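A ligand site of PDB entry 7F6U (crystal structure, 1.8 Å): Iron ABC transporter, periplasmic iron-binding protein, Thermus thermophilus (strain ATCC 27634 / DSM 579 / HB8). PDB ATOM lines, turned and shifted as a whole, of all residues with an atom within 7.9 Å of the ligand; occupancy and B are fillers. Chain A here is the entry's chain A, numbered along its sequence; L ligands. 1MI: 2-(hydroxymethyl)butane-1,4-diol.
The side-chain amide oxygen (OD1) of Asn 276 is in hydrogen-bond range of an oxygen (O1) of the ligand, at 2.5 Å.
An oxygen (O1) of the ligand sits at hydrogen-bond distance from the backbone NH (N) of Val 292 (3.0 Å).
O of Thr 290 is in hydrogen-bond range of O2 of the ligand (2.6 Å).
CD2 of Leu 272 touches C4 of the ligand, 3.5 Å away.
CA of Val 291 touches O1 of the ligand (3.6 Å).
Hydrophobic or aromatic side chains within 4 Å of the ligand: Leu 272, Val 291 and Val 292.
Of the 14 residues printed, 5 come within 4 Å of the ligand.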
ATOM      1  N   LEU A 272      -6.357 -22.168   8.677  1.00  0.00           N
ATOM      2  CA  LEU A 272      -7.684 -22.520   9.215  1.00  0.00           C
ATOM      3  C   LEU A 272      -8.458 -23.346   8.194  1.00  0.00           C
ATOM      4  O   LEU A 272      -9.165 -24.284   8.600  1.00  0.00           O
ATOM      5  CB  LEU A 272      -8.446 -21.261   9.614  1.00  0.00           C
ATOM      6  CG  LEU A 272      -9.755 -21.551  10.335  1.00  0.00           C
ATOM      7  CD1 LEU A 272      -9.504 -22.385  11.566  1.00  0.00           C
ATOM      8  CD2 LEU A 272     -10.466 -20.256  10.718  1.00  0.00           C
ATOM      9  N   ARG A 273      -8.376 -23.020   6.894  1.00  0.00           N
ATOM     10  CA  ARG A 273      -9.109 -23.851   5.902  1.00  0.00           C
ATOM     11  C   ARG A 273      -8.692 -25.316   6.017  1.00  0.00           C
ATOM     12  O   ARG A 273      -9.590 -26.189   6.186  1.00  0.00           O
ATOM     13  CB  ARG A 273      -8.859 -23.300   4.506  1.00  0.00           C
ATOM     14  CG  ARG A 273      -9.575 -24.080   3.406  1.00  0.00           C
ATOM     15  CD  ARG A 273      -9.456 -23.240   2.171  1.00  0.00           C
ATOM     16  NE  ARG A 273      -9.987 -23.977   1.051  1.00  0.00           N
ATOM     17  CZ  ARG A 273     -10.701 -23.424   0.082  1.00  0.00           C
ATOM     18  NH1 ARG A 273     -10.971 -22.121   0.084  1.00  0.00           N
ATOM     19  NH2 ARG A 273     -11.156 -24.190  -0.895  1.00  0.00           N
ATOM     20  N   GLN A 275      -6.844 -26.902   8.406  1.00  0.00           N
ATOM     21  CA  GLN A 275      -7.052 -27.426   9.790  1.00  0.00           C
ATOM     22  C   GLN A 275      -8.536 -27.725  10.007  1.00  0.00           C
ATOM     23  O   GLN A 275      -8.876 -28.782  10.570  1.00  0.00           O
ATOM     24  CB  GLN A 275      -6.515 -26.395  10.781  1.00  0.00           C
ATOM     25  CG  GLN A 275      -4.998 -26.297  10.745  1.00  0.00           C
ATOM     26  CD  GLN A 275      -4.336 -27.347  11.610  1.00  0.00           C
ATOM     27  OE1 GLN A 275      -4.629 -27.505  12.798  1.00  0.00           O
ATOM     28  NE2 GLN A 275      -3.394 -28.091  11.044  1.00  0.00           N
ATOM     29  N   ASN A 276      -9.409 -26.817   9.559  1.00  0.00           N
ATOM     30  CA  ASN A 276     -10.878 -27.042   9.647  1.00  0.00           C
ATOM     31  C   ASN A 276     -11.222 -28.353   8.926  1.00  0.00           C
ATOM     32  O   ASN A 276     -11.990 -29.139   9.420  1.00  0.00           O
ATOM     33  CB  ASN A 276     -11.666 -25.866   9.059  1.00  0.00           C
ATOM     34  CG  ASN A 276     -13.144 -26.124   9.206  1.00  0.00           C
ATOM     35  OD1 ASN A 276     -13.637 -26.256  10.314  1.00  0.00           O
ATOM     36  ND2 ASN A 276     -13.816 -26.320   8.093  1.00  0.00           N
ATOM     37  N   LEU A 277     -10.703 -28.569   7.723  1.00  0.00           N
ATOM     38  CA  LEU A 277     -11.148 -29.676   6.867  1.00  0.00           C
ATOM     39  C   LEU A 277     -10.593 -30.989   7.408  1.00  0.00           C
ATOM     40  O   LEU A 277     -11.272 -32.049   7.313  1.00  0.00           O
ATOM     41  CB  LEU A 277     -10.612 -29.400   5.462  1.00  0.00           C
ATOM     42  CG  LEU A 277     -11.129 -30.337   4.381  1.00  0.00           C
ATOM     43  CD1 LEU A 277     -12.655 -30.368   4.342  1.00  0.00           C
ATOM     44  CD2 LEU A 277     -10.561 -29.911   3.031  1.00  0.00           C
ATOM     45  N   ALA A 279      -9.933 -31.511  10.729  1.00  0.00           N
ATOM     46  CA  ALA A 279     -10.769 -31.820  11.912  1.00  0.00           C
ATOM     47  C   ALA A 279     -12.124 -32.377  11.471  1.00  0.00           C
ATOM     48  O   ALA A 279     -12.640 -33.316  12.121  1.00  0.00           O
ATOM     49  CB  ALA A 279     -10.984 -30.602  12.784  1.00  0.00           C
ATOM     50  N   TYR A 280     -12.752 -31.736  10.486  1.00  0.00           N
ATOM     51  CA  TYR A 280     -14.166 -32.011  10.106  1.00  0.00           C
ATOM     52  C   TYR A 280     -14.288 -33.305   9.279  1.00  0.00           C
ATOM     53  O   TYR A 280     -15.253 -34.114   9.446  1.00  0.00           O
ATOM     54  CB  TYR A 280     -14.712 -30.811   9.334  1.00  0.00           C
ATOM     55  CG  TYR A 280     -16.150 -30.988   8.954  1.00  0.00           C
ATOM     56  CD1 TYR A 280     -17.142 -30.729   9.874  1.00  0.00           C
ATOM     57  CD2 TYR A 280     -16.540 -31.400   7.681  1.00  0.00           C
ATOM     58  CE1 TYR A 280     -18.478 -30.900   9.575  1.00  0.00           C
ATOM     59  CE2 TYR A 280     -17.881 -31.557   7.359  1.00  0.00           C
ATOM     60  CZ  TYR A 280     -18.852 -31.319   8.320  1.00  0.00           C
ATOM     61  OH  TYR A 280     -20.180 -31.470   8.050  1.00  0.00           O
ATOM     62  N   ARG A 288      -4.585 -25.935  15.228  1.00  0.00           N
ATOM     63  CA  ARG A 288      -4.905 -24.496  15.244  1.00  0.00           C
ATOM     64  C   ARG A 288      -6.043 -24.264  16.227  1.00  0.00           C
ATOM     65  O   ARG A 288      -7.073 -24.979  16.152  1.00  0.00           O
ATOM     66  CB  ARG A 288      -5.252 -24.054  13.835  1.00  0.00           C
ATOM     67  CG  ARG A 288      -5.266 -22.560  13.645  1.00  0.00           C
ATOM     68  CD  ARG A 288      -5.570 -22.175  12.205  1.00  0.00           C
ATOM     69  NE  ARG A 288      -5.334 -20.729  12.059  1.00  0.00           N
ATOM     70  CZ  ARG A 288      -4.268 -20.207  11.430  1.00  0.00           C
ATOM     71  NH1 ARG A 288      -4.070 -18.908  11.405  1.00  0.00           N
ATOM     72  NH2 ARG A 288      -3.364 -20.977  10.864  1.00  0.00           N
ATOM     73  N   GLU A 289      -5.882 -23.281  17.091  1.00  0.00           N
ATOM     74  CA  GLU A 289      -6.782 -23.127  18.264  1.00  0.00           C
ATOM     75  C   GLU A 289      -8.141 -22.561  17.873  1.00  0.00           C
ATOM     76  O   GLU A 289      -9.032 -22.579  18.742  1.00  0.00           O
ATOM     77  CB  GLU A 289      -6.173 -22.303  19.386  1.00  0.00           C
ATOM     78  CG  GLU A 289      -5.066 -23.083  20.013  1.00  0.00           C
ATOM     79  CD  GLU A 289      -4.876 -23.142  21.504  1.00  0.00           C
ATOM     80  OE1 GLU A 289      -4.052 -24.025  21.920  1.00  0.00           O
ATOM     81  OE2 GLU A 289      -5.501 -22.295  22.230  1.00  0.00           O
ATOM     82  N   THR A 290      -8.280 -22.043  16.658  1.00  0.00           N
ATOM     83  CA  THR A 290      -9.551 -21.421  16.203  1.00  0.00           C
ATOM     84  C   THR A 290     -10.483 -22.414  15.510  1.00  0.00           C
ATOM     85  O   THR A 290     -11.586 -21.990  15.100  1.00  0.00           O
ATOM     86  CB  THR A 290      -9.220 -20.210  15.321  1.00  0.00           C
ATOM     87  OG1 THR A 290      -8.291 -20.649  14.317  1.00  0.00           O
ATOM     88  CG2 THR A 290      -8.669 -19.114  16.203  1.00  0.00           C
ATOM     89  N   VAL A 291     -10.092 -23.682  15.381  1.00  0.00           N
ATOM     90  CA  VAL A 291     -10.989 -24.664  14.694  1.00  0.00           C
ATOM     91  C   VAL A 291     -12.168 -25.009  15.613  1.00  0.00           C
ATOM     92  O   VAL A 291     -11.947 -25.324  16.801  1.00  0.00           O
ATOM     93  CB  VAL A 291     -10.240 -25.945  14.276  1.00  0.00           C
ATOM     94  CG1 VAL A 291     -11.125 -26.854  13.470  1.00  0.00           C
ATOM     95  CG2 VAL A 291      -8.991 -25.593  13.490  1.00  0.00           C
ATOM     96  N   VAL A 292     -13.356 -25.054  15.032  1.00  0.00           N
ATOM     97  CA  VAL A 292     -14.631 -25.381  15.720  1.00  0.00           C
ATOM     98  C   VAL A 292     -15.009 -26.821  15.389  1.00  0.00           C
ATOM     99  O   VAL A 292     -15.213 -27.152  14.191  1.00  0.00           O
ATOM    100  CB  VAL A 292     -15.744 -24.404  15.335  1.00  0.00           C
ATOM    101  CG1 VAL A 292     -17.059 -24.771  16.033  1.00  0.00           C
ATOM    102  CG2 VAL A 292     -15.337 -22.967  15.656  1.00  0.00           C
ATOM    103  N   GLY A 293     -15.127 -27.653  16.404  1.00  0.00           N
ATOM    104  CA  GLY A 293     -15.608 -29.036  16.231  1.00  0.00           C
ATOM    105  C   GLY A 293     -14.989 -29.971  17.234  1.00  0.00           C
ATOM    106  O   GLY A 293     -14.216 -29.499  18.103  1.00  0.00           O
ATOM    107  N   THR A 296     -10.641 -30.888  18.036  1.00  0.00           N
ATOM    108  CA  THR A 296     -10.018 -29.560  18.069  1.00  0.00           C
ATOM    109  C   THR A 296      -9.433 -29.267  19.430  1.00  0.00           C
ATOM    110  O   THR A 296      -9.898 -29.804  20.449  1.00  0.00           O
ATOM    111  CB  THR A 296     -11.030 -28.447  17.747  1.00  0.00           C
ATOM    112  OG1 THR A 296     -11.995 -28.364  18.804  1.00  0.00           O
ATOM    113  CG2 THR A 296     -11.773 -28.675  16.442  1.00  0.00           C
HETATM  114  C1  1MI L   1     -14.530 -20.811  12.275  1.00  0.00           C
HETATM  115  C2  1MI L   1     -15.720 -22.913  11.634  1.00  0.00           C
HETATM  116  C3  1MI L   1     -13.252 -23.034  12.128  1.00  0.00           C
HETATM  117  C4  1MI L   1     -13.229 -20.196  12.819  1.00  0.00           C
HETATM  118  O2  1MI L   1     -13.164 -20.050  14.242  1.00  0.00           O
HETATM  119  C   1MI L   1     -14.396 -22.163  11.561  1.00  0.00           C
HETATM  120  O1  1MI L   1     -13.503 -24.435  12.083  1.00  0.00           O
HETATM  121  O   1MI L   1     -16.827 -22.010  11.432  1.00  0.00           O
